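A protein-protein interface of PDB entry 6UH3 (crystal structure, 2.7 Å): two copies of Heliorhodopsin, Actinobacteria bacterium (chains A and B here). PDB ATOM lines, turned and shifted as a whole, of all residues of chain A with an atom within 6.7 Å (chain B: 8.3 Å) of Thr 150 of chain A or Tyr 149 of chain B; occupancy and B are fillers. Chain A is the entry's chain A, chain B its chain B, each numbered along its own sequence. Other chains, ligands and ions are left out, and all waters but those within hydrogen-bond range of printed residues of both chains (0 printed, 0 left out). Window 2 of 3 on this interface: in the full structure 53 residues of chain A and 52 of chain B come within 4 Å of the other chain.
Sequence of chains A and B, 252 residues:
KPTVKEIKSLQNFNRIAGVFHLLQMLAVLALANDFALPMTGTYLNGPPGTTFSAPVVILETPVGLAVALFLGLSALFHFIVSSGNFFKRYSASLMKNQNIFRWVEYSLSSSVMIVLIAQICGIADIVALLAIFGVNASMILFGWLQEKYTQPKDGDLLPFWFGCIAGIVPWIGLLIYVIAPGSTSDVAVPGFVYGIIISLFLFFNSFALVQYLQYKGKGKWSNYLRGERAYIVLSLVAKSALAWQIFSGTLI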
ATOM      1  N   LYS A  96      12.980  -4.959 -11.184  1.00  0.00           N
ATOM      2  CA  LYS A  96      12.209  -3.762 -10.861  1.00  0.00           C
ATOM      3  C   LYS A  96      11.949  -3.584  -9.389  1.00  0.00           C
ATOM      4  O   LYS A  96      12.161  -4.484  -8.576  1.00  0.00           O
ATOM      5  CB  LYS A  96      10.872  -3.754 -11.604  1.00  0.00           C
ATOM      6  CG  LYS A  96      11.015  -3.643 -13.110  1.00  0.00           C
ATOM      7  CD  LYS A  96      11.748  -2.348 -13.464  1.00  0.00           C
ATOM      8  CE  LYS A  96      11.695  -2.033 -14.949  1.00  0.00           C
ATOM      9  NZ  LYS A  96      12.501  -0.828 -15.313  1.00  0.00           N
ATOM     10  N   GLN A  98       9.448  -2.923  -6.157  1.00  0.00           N
ATOM     11  CA  GLN A  98       8.187  -3.474  -5.715  1.00  0.00           C
ATOM     12  C   GLN A  98       7.678  -2.503  -4.675  1.00  0.00           C
ATOM     13  O   GLN A  98       8.469  -1.893  -3.951  1.00  0.00           O
ATOM     14  CB  GLN A  98       8.366  -4.885  -5.140  1.00  0.00           C
ATOM     15  CG  GLN A  98       8.928  -5.882  -6.148  1.00  0.00           C
ATOM     16  CD  GLN A  98       9.058  -7.285  -5.593  1.00  0.00           C
ATOM     17  OE1 GLN A  98       8.643  -7.563  -4.473  1.00  0.00           O
ATOM     18  NE2 GLN A  98       9.638  -8.178  -6.379  1.00  0.00           N
ATOM     19  N   LEU A 145       1.154  -9.915  -6.018  1.00  0.00           N
ATOM     20  CA  LEU A 145       1.859 -11.130  -6.437  1.00  0.00           C
ATOM     21  C   LEU A 145       2.456 -11.011  -7.835  1.00  0.00           C
ATOM     22  O   LEU A 145       3.525 -11.574  -8.097  1.00  0.00           O
ATOM     23  CB  LEU A 145       0.933 -12.341  -6.361  1.00  0.00           C
ATOM     24  CG  LEU A 145       0.516 -12.815  -4.959  1.00  0.00           C
ATOM     25  CD1 LEU A 145      -0.402 -14.035  -5.013  1.00  0.00           C
ATOM     26  CD2 LEU A 145       1.758 -13.138  -4.145  1.00  0.00           C
ATOM     27  N   GLN A 146       1.797 -10.282  -8.736  1.00  0.00           N
ATOM     28  CA  GLN A 146       2.388  -9.970 -10.037  1.00  0.00           C
ATOM     29  C   GLN A 146       3.727  -9.292  -9.873  1.00  0.00           C
ATOM     30  O   GLN A 146       4.715  -9.630 -10.535  1.00  0.00           O
ATOM     31  CB  GLN A 146       1.489  -9.016 -10.798  1.00  0.00           C
ATOM     32  CG  GLN A 146       1.963  -8.726 -12.193  1.00  0.00           C
ATOM     33  CD  GLN A 146       1.099  -7.702 -12.838  1.00  0.00           C
ATOM     34  OE1 GLN A 146       0.200  -7.180 -12.190  1.00  0.00           O
ATOM     35  NE2 GLN A 146       1.340  -7.408 -14.107  1.00  0.00           N
ATOM     36  N   GLU A 147       3.743  -8.269  -9.036  1.00  0.00           N
ATOM     37  CA  GLU A 147       4.931  -7.470  -8.833  1.00  0.00           C
ATOM     38  C   GLU A 147       6.007  -8.266  -8.101  1.00  0.00           C
ATOM     39  O   GLU A 147       7.195  -8.133  -8.410  1.00  0.00           O
ATOM     40  CB  GLU A 147       4.521  -6.197  -8.098  1.00  0.00           C
ATOM     41  CG  GLU A 147       5.520  -5.099  -8.155  1.00  0.00           C
ATOM     42  CD  GLU A 147       4.915  -3.795  -7.722  1.00  0.00           C
ATOM     43  OE1 GLU A 147       4.594  -3.643  -6.530  1.00  0.00           O
ATOM     44  OE2 GLU A 147       4.727  -2.929  -8.588  1.00  0.00           O
ATOM     45  N   LYS A 148       5.598  -9.114  -7.148  1.00  0.00           N
ATOM     46  CA  LYS A 148       6.538  -9.951  -6.398  1.00  0.00           C
ATOM     47  C   LYS A 148       7.269 -10.975  -7.254  1.00  0.00           C
ATOM     48  O   LYS A 148       8.489 -11.138  -7.134  1.00  0.00           O
ATOM     49  CB  LYS A 148       5.813 -10.707  -5.287  1.00  0.00           C
ATOM     50  CG  LYS A 148       6.755 -11.620  -4.483  1.00  0.00           C
ATOM     51  CD  LYS A 148       6.048 -12.335  -3.339  1.00  0.00           C
ATOM     52  CE  LYS A 148       6.973 -13.294  -2.577  1.00  0.00           C
ATOM     53  NZ  LYS A 148       7.934 -12.600  -1.678  1.00  0.00           N
ATOM     54  N   TYR A 149       6.547 -11.706  -8.097  1.00  0.00           N
ATOM     55  CA  TYR A 149       7.187 -12.838  -8.754  1.00  0.00           C
ATOM     56  C   TYR A 149       7.595 -12.619 -10.197  1.00  0.00           C
ATOM     57  O   TYR A 149       8.281 -13.486 -10.750  1.00  0.00           O
ATOM     58  CB  TYR A 149       6.280 -14.080  -8.691  1.00  0.00           C
ATOM     59  CG  TYR A 149       6.076 -14.627  -7.287  1.00  0.00           C
ATOM     60  CD1 TYR A 149       4.811 -14.644  -6.710  1.00  0.00           C
ATOM     61  CD2 TYR A 149       7.142 -15.139  -6.562  1.00  0.00           C
ATOM     62  CE1 TYR A 149       4.613 -15.153  -5.442  1.00  0.00           C
ATOM     63  CE2 TYR A 149       6.953 -15.650  -5.295  1.00  0.00           C
ATOM     64  CZ  TYR A 149       5.685 -15.651  -4.738  1.00  0.00           C
ATOM     65  OH  TYR A 149       5.492 -16.149  -3.468  1.00  0.00           O
ATOM     66  N   THR A 150       7.214 -11.523 -10.835  1.00  0.00           N
ATOM     67  CA  THR A 150       7.599 -11.361 -12.224  1.00  0.00           C
ATOM     68  C   THR A 150       8.199  -9.994 -12.512  1.00  0.00           C
ATOM     69  O   THR A 150       8.033  -9.028 -11.762  1.00  0.00           O
ATOM     70  CB  THR A 150       6.404 -11.563 -13.156  1.00  0.00           C
ATOM     71  OG1 THR A 150       5.498 -10.457 -13.013  1.00  0.00           O
ATOM     72  CG2 THR A 150       5.678 -12.858 -12.838  1.00  0.00           C
ATOM     73  N   GLN A 151       8.879  -9.940 -13.647  1.00  0.00           N
ATOM     74  CA  GLN A 151       9.470  -8.732 -14.182  1.00  0.00           C
ATOM     75  C   GLN A 151       8.657  -8.343 -15.409  1.00  0.00           C
ATOM     76  O   GLN A 151       7.719  -9.060 -15.783  1.00  0.00           O
ATOM     77  CB  GLN A 151      10.945  -8.977 -14.527  1.00  0.00           C
ATOM     78  CG  GLN A 151      11.810  -9.337 -13.330  1.00  0.00           C
ATOM     79  CD  GLN A 151      11.897  -8.211 -12.331  1.00  0.00           C
ATOM     80  OE1 GLN A 151      11.697  -8.367 -11.185  1.00  0.00           O
ATOM     81  NE2 GLN A 151      12.184  -7.086 -12.785  1.00  0.00           N
ATOM     82  N   PRO A 152       8.968  -7.228 -16.043  1.00  0.00           N
ATOM     83  CA  PRO A 152       8.256  -6.854 -17.265  1.00  0.00           C
ATOM     84  C   PRO A 152       8.598  -7.764 -18.430  1.00  0.00           C
ATOM     85  O   PRO A 152       9.419  -7.444 -19.298  1.00  0.00           O
ATOM     86  CB  PRO A 152       8.705  -5.409 -17.490  1.00  0.00           C
ATOM     87  CG  PRO A 152       8.839  -4.872 -16.091  1.00  0.00           C
ATOM     88  CD  PRO A 152       9.349  -6.045 -15.253  1.00  0.00           C
ATOM     89  N   LYS A 153       7.922  -8.914 -18.430  1.00  0.00           N
ATOM     90  CA  LYS A 153       8.087 -10.012 -19.372  1.00  0.00           C
ATOM     91  C   LYS A 153       6.793 -10.813 -19.355  1.00  0.00           C
ATOM     92  O   LYS A 153       5.963 -10.655 -18.457  1.00  0.00           O
ATOM     93  CB  LYS A 153       9.275 -10.887 -18.986  1.00  0.00           C
ATOM     94  CG  LYS A 153       9.069 -11.565 -17.645  1.00  0.00           C
ATOM     95  CD  LYS A 153      10.306 -12.315 -17.219  1.00  0.00           C
ATOM     96  CE  LYS A 153      10.118 -12.932 -15.848  1.00  0.00           C
ATOM     97  NZ  LYS A 153      11.346 -13.645 -15.427  1.00  0.00           N
ATOM     98  N   ASP A 154       6.642 -11.688 -20.354  1.00  0.00           N
ATOM     99  CA  ASP A 154       5.431 -12.479 -20.579  1.00  0.00           C
ATOM    100  C   ASP A 154       4.829 -13.101 -19.318  1.00  0.00           C
ATOM    101  O   ASP A 154       3.605 -13.110 -19.146  1.00  0.00           O
ATOM    102  CB  ASP A 154       5.725 -13.612 -21.566  1.00  0.00           C
ATOM    103  CG  ASP A 154       6.036 -13.118 -22.965  1.00  0.00           C
ATOM    104  OD1 ASP A 154       5.833 -11.922 -23.248  1.00  0.00           O
ATOM    105  OD2 ASP A 154       6.482 -13.931 -23.796  1.00  0.00           O
ATOM    106  N   GLY A 155       5.678 -13.589 -18.412  1.00  0.00           N
ATOM    107  CA  GLY A 155       5.252 -14.346 -17.238  1.00  0.00           C
ATOM    108  C   GLY A 155       4.334 -13.611 -16.267  1.00  0.00           C
ATOM    109  O   GLY A 155       3.757 -14.261 -15.387  1.00  0.00           O
ATOM    110  N   ASP A 156       4.170 -12.292 -16.408  1.00  0.00           N
ATOM    111  CA  ASP A 156       3.347 -11.514 -15.481  1.00  0.00           C
ATOM    112  C   ASP A 156       1.858 -11.629 -15.766  1.00  0.00           C
ATOM    113  O   ASP A 156       1.052 -11.109 -14.979  1.00  0.00           O
ATOM    114  CB  ASP A 156       3.698 -10.027 -15.548  1.00  0.00           C
ATOM    115  CG  ASP A 156       3.138  -9.369 -16.790  1.00  0.00           C
ATOM    116  OD1 ASP A 156       3.338  -9.897 -17.899  1.00  0.00           O
ATOM    117  OD2 ASP A 156       2.453  -8.341 -16.648  1.00  0.00           O
ATOM    118  N   LEU A 157       1.492 -12.268 -16.879  1.00  0.00           N
ATOM    119  CA  LEU A 157       0.105 -12.352 -17.321  1.00  0.00           C
ATOM    120  C   LEU A 157      -0.838 -12.824 -16.225  1.00  0.00           C
ATOM    121  O   LEU A 157      -1.777 -12.110 -15.852  1.00  0.00           O
ATOM    122  CB  LEU A 157       0.051 -13.320 -18.497  1.00  0.00           C
ATOM    123  CG  LEU A 157       0.615 -12.770 -19.786  1.00  0.00           C
ATOM    124  CD1 LEU A 157       0.753 -13.912 -20.752  1.00  0.00           C
ATOM    125  CD2 LEU A 157      -0.363 -11.741 -20.322  1.00  0.00           C
ATOM    126  N   LEU A 158      -0.585 -14.015 -15.671  1.00  0.00           N
ATOM    127  CA  LEU A 158      -1.597 -14.632 -14.816  1.00  0.00           C
ATOM    128  C   LEU A 158      -1.965 -13.808 -13.601  1.00  0.00           C
ATOM    129  O   LEU A 158      -3.140 -13.423 -13.475  1.00  0.00           O
ATOM    130  CB  LEU A 158      -1.156 -16.022 -14.372  1.00  0.00           C
ATOM    131  CG  LEU A 158      -1.786 -17.124 -15.180  1.00  0.00           C
ATOM    132  CD1 LEU A 158      -1.402 -16.947 -16.630  1.00  0.00           C
ATOM    133  CD2 LEU A 158      -1.322 -18.429 -14.603  1.00  0.00           C
ATOM    134  N   PRO A 159      -1.040 -13.523 -12.668  1.00  0.00           N
ATOM    135  CA  PRO A 159      -1.375 -12.729 -11.484  1.00  0.00           C
ATOM    136  C   PRO A 159      -2.236 -11.526 -11.821  1.00  0.00           C
ATOM    137  O   PRO A 159      -3.258 -11.276 -11.168  1.00  0.00           O
ATOM    138  CB  PRO A 159       0.001 -12.314 -10.963  1.00  0.00           C
ATOM    139  CG  PRO A 159       0.911 -13.416 -11.407  1.00  0.00           C
ATOM    140  CD  PRO A 159       0.422 -13.701 -12.784  1.00  0.00           C
ATOM    141  N   TYR A 215       4.307  -3.248 -16.750  1.00  0.00           N
ATOM    142  CA  TYR A 215       4.819  -4.585 -17.014  1.00  0.00           C
ATOM    143  C   TYR A 215       4.893  -4.920 -18.497  1.00  0.00           C
ATOM    144  O   TYR A 215       5.736  -5.734 -18.893  1.00  0.00           O
ATOM    145  CB  TYR A 215       4.000  -5.612 -16.222  1.00  0.00           C
ATOM    146  CG  TYR A 215       4.599  -5.690 -14.853  1.00  0.00           C
ATOM    147  CD1 TYR A 215       4.209  -4.822 -13.844  1.00  0.00           C
ATOM    148  CD2 TYR A 215       5.655  -6.549 -14.624  1.00  0.00           C
ATOM    149  CE1 TYR A 215       4.812  -4.878 -12.603  1.00  0.00           C
ATOM    150  CE2 TYR A 215       6.271  -6.603 -13.414  1.00  0.00           C
ATOM    151  CZ  TYR A 215       5.857  -5.781 -12.398  1.00  0.00           C
ATOM    152  OH  TYR A 215       6.527  -5.849 -11.196  1.00  0.00           O
ATOM    153  N   GLN B  98       2.803 -29.267 -10.631  1.00  0.00           N
ATOM    154  CA  GLN B  98       1.660 -28.378 -10.666  1.00  0.00           C
ATOM    155  C   GLN B  98       0.458 -29.155 -11.165  1.00  0.00           C
ATOM    156  O   GLN B  98       0.604 -30.134 -11.899  1.00  0.00           O
ATOM    157  CB  GLN B  98       1.930 -27.189 -11.591  1.00  0.00           C
ATOM    158  CG  GLN B  98       3.087 -26.329 -11.135  1.00  0.00           C
ATOM    159  CD  GLN B  98       3.526 -25.344 -12.185  1.00  0.00           C
ATOM    160  OE1 GLN B  98       3.056 -25.378 -13.315  1.00  0.00           O
ATOM    161  NE2 GLN B  98       4.453 -24.473 -11.823  1.00  0.00           N
ATOM    162  N   LEU B 141      -7.392 -19.487  -6.926  1.00  0.00           N
ATOM    163  CA  LEU B 141      -6.402 -18.864  -7.795  1.00  0.00           C
ATOM    164  C   LEU B 141      -5.134 -18.482  -7.046  1.00  0.00           C
ATOM    165  O   LEU B 141      -4.044 -18.491  -7.631  1.00  0.00           O
ATOM    166  CB  LEU B 141      -7.006 -17.629  -8.456  1.00  0.00           C
ATOM    167  CG  LEU B 141      -8.132 -17.905  -9.439  1.00  0.00           C
ATOM    168  CD1 LEU B 141      -8.656 -16.622 -10.045  1.00  0.00           C
ATOM    169  CD2 LEU B 141      -7.604 -18.812 -10.527  1.00  0.00           C
ATOM    170  N   PHE B 142      -5.241 -18.101  -5.774  1.00  0.00           N
ATOM    171  CA  PHE B 142      -4.025 -17.870  -5.006  1.00  0.00           C
ATOM    172  C   PHE B 142      -3.242 -19.168  -4.846  1.00  0.00           C
ATOM    173  O   PHE B 142      -2.018 -19.190  -5.024  1.00  0.00           O
ATOM    174  CB  PHE B 142      -4.362 -17.268  -3.637  1.00  0.00           C
ATOM    175  CG  PHE B 142      -4.656 -15.794  -3.669  1.00  0.00           C
ATOM    176  CD1 PHE B 142      -5.867 -15.308  -3.213  1.00  0.00           C
ATOM    177  CD2 PHE B 142      -3.722 -14.896  -4.147  1.00  0.00           C
ATOM    178  CE1 PHE B 142      -6.142 -13.962  -3.236  1.00  0.00           C
ATOM    179  CE2 PHE B 142      -3.994 -13.531  -4.173  1.00  0.00           C
ATOM    180  CZ  PHE B 142      -5.209 -13.072  -3.717  1.00  0.00           C
ATOM    181  N   GLY B 143      -3.943 -20.264  -4.554  1.00  0.00           N
ATOM    182  CA  GLY B 143      -3.287 -21.559  -4.432  1.00  0.00           C
ATOM    183  C   GLY B 143      -2.600 -22.001  -5.707  1.00  0.00           C
ATOM    184  O   GLY B 143      -1.500 -22.555  -5.676  1.00  0.00           O
ATOM    185  N   TRP B 144      -3.270 -21.806  -6.836  1.00  0.00           N
ATOM    186  CA  TRP B 144      -2.660 -21.983  -8.148  1.00  0.00           C
ATOM    187  C   TRP B 144      -1.336 -21.233  -8.250  1.00  0.00           C
ATOM    188  O   TRP B 144      -0.332 -21.801  -8.689  1.00  0.00           O
ATOM    189  CB  TRP B 144      -3.667 -21.523  -9.216  1.00  0.00           C
ATOM    190  CG  TRP B 144      -3.228 -21.537 -10.647  1.00  0.00           C
ATOM    191  CD1 TRP B 144      -1.953 -21.516 -11.124  1.00  0.00           C
ATOM    192  CD2 TRP B 144      -4.083 -21.540 -11.796  1.00  0.00           C
ATOM    193  NE1 TRP B 144      -1.956 -21.520 -12.491  1.00  0.00           N
ATOM    194  CE2 TRP B 144      -3.250 -21.527 -12.935  1.00  0.00           C
ATOM    195  CE3 TRP B 144      -5.471 -21.557 -11.974  1.00  0.00           C
ATOM    196  CZ2 TRP B 144      -3.755 -21.526 -14.234  1.00  0.00           C
ATOM    197  CZ3 TRP B 144      -5.971 -21.561 -13.270  1.00  0.00           C
ATOM    198  CH2 TRP B 144      -5.116 -21.544 -14.381  1.00  0.00           C
ATOM    199  N   LEU B 145      -1.313 -19.958  -7.843  1.00  0.00           N
ATOM    200  CA  LEU B 145      -0.084 -19.165  -7.917  1.00  0.00           C
ATOM    201  C   LEU B 145       1.009 -19.699  -6.998  1.00  0.00           C
ATOM    202  O   LEU B 145       2.196 -19.638  -7.343  1.00  0.00           O
ATOM    203  CB  LEU B 145      -0.398 -17.707  -7.580  1.00  0.00           C
ATOM    204  CG  LEU B 145      -1.312 -16.960  -8.568  1.00  0.00           C
ATOM    205  CD1 LEU B 145      -1.665 -15.571  -8.055  1.00  0.00           C
ATOM    206  CD2 LEU B 145      -0.644 -16.827  -9.921  1.00  0.00           C
ATOM    207  N   GLN B 146       0.632 -20.257  -5.851  1.00  0.00           N
ATOM    208  CA  GLN B 146       1.599 -20.920  -4.985  1.00  0.00           C
ATOM    209  C   GLN B 146       2.343 -22.025  -5.720  1.00  0.00           C
ATOM    210  O   GLN B 146       3.570 -22.144  -5.618  1.00  0.00           O
ATOM    211  CB  GLN B 146       0.866 -21.513  -3.795  1.00  0.00           C
ATOM    212  CG  GLN B 146       1.749 -22.137  -2.749  1.00  0.00           C
ATOM    213  CD  GLN B 146       0.933 -22.807  -1.716  1.00  0.00           C
ATOM    214  OE1 GLN B 146      -0.291 -22.776  -1.791  1.00  0.00           O
ATOM    215  NE2 GLN B 146       1.577 -23.441  -0.759  1.00  0.00           N
ATOM    216  N   GLU B 147       1.604 -22.853  -6.459  1.00  0.00           N
ATOM    217  CA  GLU B 147       2.229 -23.916  -7.238  1.00  0.00           C
ATOM    218  C   GLU B 147       2.997 -23.380  -8.438  1.00  0.00           C
ATOM    219  O   GLU B 147       4.008 -23.973  -8.835  1.00  0.00           O
ATOM    220  CB  GLU B 147       1.171 -24.918  -7.699  1.00  0.00           C
ATOM    221  CG  GLU B 147       0.546 -25.778  -6.598  1.00  0.00           C
ATOM    222  CD  GLU B 147      -0.114 -27.015  -7.132  1.00  0.00           C
ATOM    223  OE1 GLU B 147      -0.620 -26.982  -8.262  1.00  0.00           O
ATOM    224  OE2 GLU B 147      -0.132 -28.036  -6.434  1.00  0.00           O
ATOM    225  N   LYS B 148       2.522 -22.284  -9.037  1.00  0.00           N
ATOM    226  CA  LYS B 148       3.154 -21.745 -10.239  1.00  0.00           C
ATOM    227  C   LYS B 148       4.526 -21.133  -9.985  1.00  0.00           C
ATOM    228  O   LYS B 148       5.495 -21.458 -10.679  1.00  0.00           O
ATOM    229  CB  LYS B 148       2.252 -20.701 -10.890  1.00  0.00           C
ATOM    230  CG  LYS B 148       2.830 -20.175 -12.208  1.00  0.00           C
ATOM    231  CD  LYS B 148       1.863 -19.312 -12.980  1.00  0.00           C
ATOM    232  CE  LYS B 148       2.469 -18.873 -14.304  1.00  0.00           C
ATOM    233  NZ  LYS B 148       2.448 -19.979 -15.305  1.00  0.00           N
ATOM    234  N   TYR B 149       4.632 -20.240  -9.008  1.00  0.00           N
ATOM    235  CA  TYR B 149       5.866 -19.493  -8.815  1.00  0.00           C
ATOM    236  C   TYR B 149       6.722 -19.968  -7.650  1.00  0.00           C
ATOM    237  O   TYR B 149       7.766 -19.357  -7.394  1.00  0.00           O
ATOM    238  CB  TYR B 149       5.527 -17.995  -8.652  1.00  0.00           C
ATOM    239  CG  TYR B 149       4.869 -17.385  -9.901  1.00  0.00           C
ATOM    240  CD1 TYR B 149       3.513 -17.073  -9.917  1.00  0.00           C
ATOM    241  CD2 TYR B 149       5.591 -17.190 -11.071  1.00  0.00           C
ATOM    242  CE1 TYR B 149       2.908 -16.529 -11.063  1.00  0.00           C
ATOM    243  CE2 TYR B 149       4.986 -16.650 -12.211  1.00  0.00           C
ATOM    244  CZ  TYR B 149       3.653 -16.323 -12.200  1.00  0.00           C
ATOM    245  OH  TYR B 149       3.064 -15.813 -13.333  1.00  0.00           O
ATOM    246  N   THR B 150       6.337 -21.018  -6.923  1.00  0.00           N
ATOM    247  CA  THR B 150       7.153 -21.424  -5.782  1.00  0.00           C
ATOM    248  C   THR B 150       7.309 -22.942  -5.669  1.00  0.00           C
ATOM    249  O   THR B 150       6.599 -23.730  -6.302  1.00  0.00           O
ATOM    250  CB  THR B 150       6.572 -20.858  -4.486  1.00  0.00           C
ATOM    251  OG1 THR B 150       5.312 -21.479  -4.224  1.00  0.00           O
ATOM    252  CG2 THR B 150       6.373 -19.335  -4.581  1.00  0.00           C
ATOM    253  N   GLN B 151       8.288 -23.340  -4.835  1.00  0.00           N
ATOM    254  CA  GLN B 151       8.683 -24.709  -4.501  1.00  0.00           C
ATOM    255  C   GLN B 151       8.719 -24.835  -2.977  1.00  0.00           C
ATOM    256  O   GLN B 151       8.239 -23.931  -2.283  1.00  0.00           O
ATOM    257  CB  GLN B 151      10.044 -25.030  -5.130  1.00  0.00           C
ATOM    258  CG  GLN B 151      10.010 -25.176  -6.639  1.00  0.00           C
ATOM    259  CD  GLN B 151       9.379 -26.477  -7.085  1.00  0.00           C
ATOM    260  OE1 GLN B 151       8.512 -26.497  -7.873  1.00  0.00           O
ATOM    261  NE2 GLN B 151       9.817 -27.537  -6.584  1.00  0.00           N
ATOM    262  N   LYS B 153      10.100 -23.835  -0.233  1.00  0.00           N
ATOM    263  CA  LYS B 153      10.971 -22.760   0.230  1.00  0.00           C
ATOM    264  C   LYS B 153      10.122 -21.704   0.932  1.00  0.00           C
ATOM    265  O   LYS B 153       8.898 -21.689   0.787  1.00  0.00           O
ATOM    266  CB  LYS B 153      11.708 -22.125  -0.945  1.00  0.00           C
ATOM    267  CG  LYS B 153      10.751 -21.462  -1.937  1.00  0.00           C
ATOM    268  CD  LYS B 153      11.500 -20.840  -3.102  1.00  0.00           C
ATOM    269  CE  LYS B 153      10.578 -20.060  -4.021  1.00  0.00           C
ATOM    270  NZ  LYS B 153      11.349 -19.400  -5.113  1.00  0.00           N
ATOM    271  N   GLY B 155       9.576 -18.554   0.411  1.00  0.00           N
ATOM    272  CA  GLY B 155       8.813 -17.715  -0.516  1.00  0.00           C
ATOM    273  C   GLY B 155       7.510 -18.322  -1.007  1.00  0.00           C
ATOM    274  O   GLY B 155       6.737 -17.634  -1.687  1.00  0.00           O
ATOM    275  N   ASP B 156       7.275 -19.602  -0.700  1.00  0.00           N
ATOM    276  CA  ASP B 156       6.039 -20.307  -1.034  1.00  0.00           C
ATOM    277  C   ASP B 156       4.845 -19.836  -0.216  1.00  0.00           C
ATOM    278  O   ASP B 156       3.699 -19.958  -0.670  1.00  0.00           O
ATOM    279  CB  ASP B 156       6.240 -21.802  -0.779  1.00  0.00           C
ATOM    280  CG  ASP B 156       5.041 -22.641  -1.157  1.00  0.00           C
ATOM    281  OD1 ASP B 156       4.863 -22.957  -2.346  1.00  0.00           O
ATOM    282  OD2 ASP B 156       4.263 -22.989  -0.248  1.00  0.00           O
ATOM    283  N   PRO B 159       1.414 -16.615  -1.378  1.00  0.00           N
ATOM    284  CA  PRO B 159       0.158 -16.956  -2.077  1.00  0.00           C
ATOM    285  C   PRO B 159      -0.768 -17.794  -1.225  1.00  0.00           C
ATOM    286  O   PRO B 159      -1.996 -17.626  -1.269  1.00  0.00           O
ATOM    287  CB  PRO B 159       0.648 -17.734  -3.299  1.00  0.00           C
ATOM    288  CG  PRO B 159       2.027 -17.231  -3.525  1.00  0.00           C
ATOM    289  CD  PRO B 159       2.585 -17.045  -2.150  1.00  0.00           C
ATOM    290  N   TYR B 215       4.010 -28.361   0.477  1.00  0.00           N
ATOM    291  CA  TYR B 215       5.059 -27.382   0.236  1.00  0.00           C
ATOM    292  C   TYR B 215       5.918 -27.119   1.455  1.00  0.00           C
ATOM    293  O   TYR B 215       7.055 -26.661   1.309  1.00  0.00           O
ATOM    294  CB  TYR B 215       4.445 -26.099  -0.296  1.00  0.00           C
ATOM    295  CG  TYR B 215       4.217 -26.235  -1.768  1.00  0.00           C
ATOM    296  CD1 TYR B 215       2.960 -26.525  -2.277  1.00  0.00           C
ATOM    297  CD2 TYR B 215       5.283 -26.124  -2.636  1.00  0.00           C
ATOM    298  CE1 TYR B 215       2.768 -26.668  -3.636  1.00  0.00           C
ATOM    299  CE2 TYR B 215       5.108 -26.266  -3.981  1.00  0.00           C
ATOM    300  CZ  TYR B 215       3.853 -26.534  -4.484  1.00  0.00           C
ATOM    301  OH  TYR B 215       3.707 -26.683  -5.846  1.00  0.00           O
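The side-chain hydroxyl of Thr 150 of chain A is in hydrogen-bond range of the backbone carbonyl oxygen of Gln 146 of chain A. NE2 of Gln 98 of chain B sits at hydrogen-bond distance from O of Lys 148 of chain B (3.4 Å). The side-chain hydroxyl (OG1) of Thr 150 of chain B is in hydrogen-bond range of the side-chain carboxylate (OD1) of Asp 156 of chain B, 2.4 Å away.
OH of Tyr 149 of chain A lies within hydrogen-bond range of O of Gly 155 of chain B. The side-chain hydroxyl (OH) of Tyr 149 of chain B lies within hydrogen-bond range of the backbone carbonyl oxygen (O) of Gly 155 of chain A (2.7 Å).
Leu 145 of chain A touches Phe 142 of chain B. Leu 145 of chain A touches Leu 145 of chain B (CD1 to CD1, 3.6 Å). Tyr 149 of chain A touches Tyr 149 of chain B. OH of Tyr 149 of chain A touches CG2 of Thr 150 of chain B, 3.5 Å away. OH of Tyr 149 of chain A touches CD of Pro 159 of chain B (3.3 Å). Thr 150 of chain A touches Tyr 149 of chain B. Leu 158 of chain A touches Trp 144 of chain B. Lys 148 of chain B touches Leu 158 of chain A. Pro 159 of chain A touches Tyr 149 of chain B (CD to OH, 3.4 Å).
Of the 17 printed residues of chain B, 8 touch a printed residue of chain A. Of the 18 printed residues of chain A, 6 touch a printed residue of chain B. Hydrophobic or aromatic side chains of chain A that line the printed part of chain B: Leu 145, Tyr 149, Leu 158 and Pro 159.
Leu 145 of chain B touches its own counterpart, Leu 145 of chain A. Tyr 149 of chain A touches its own counterpart, Tyr 149 of chain B. Tyr 149 of chain A touches Gly 155 of chain B, and with the chains exchanged Gly 155 of chain A touches Tyr 149 of chain B. Tyr 149 of chain A touches Pro 159 of chain B, and with the chains exchanged Pro 159 of chain A touches Tyr 149 of chain B. 13 positions are printed for both chains. Of the 11 pairs that touch across the chains among the printed residues, 8 have their exchanged pair printed and touching as well.
Thr 150 of chain A touches just one residue of chain B: Tyr 149. Pro 152 of chain A touches none of the printed residues of chain B. Of the printed residues of chain B, Leu 158 of chain A touches Trp 144 (3.8 Å) and Lys 148 (3.7 Å). Of chain A, only Tyr 149 (3.7 Å), Thr 150 (3.9 Å), Gly 155 (2.7 Å) and Pro 159 (3.4 Å) come within 4 Å of Tyr 149 of chain B. Of the printed residues of chain A, Pro 159 of chain B touches Tyr 149. The nearest printed residue of chain A that does not touch Pro 159 of chain B is Leu 145 of chain A (4.1 Å).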
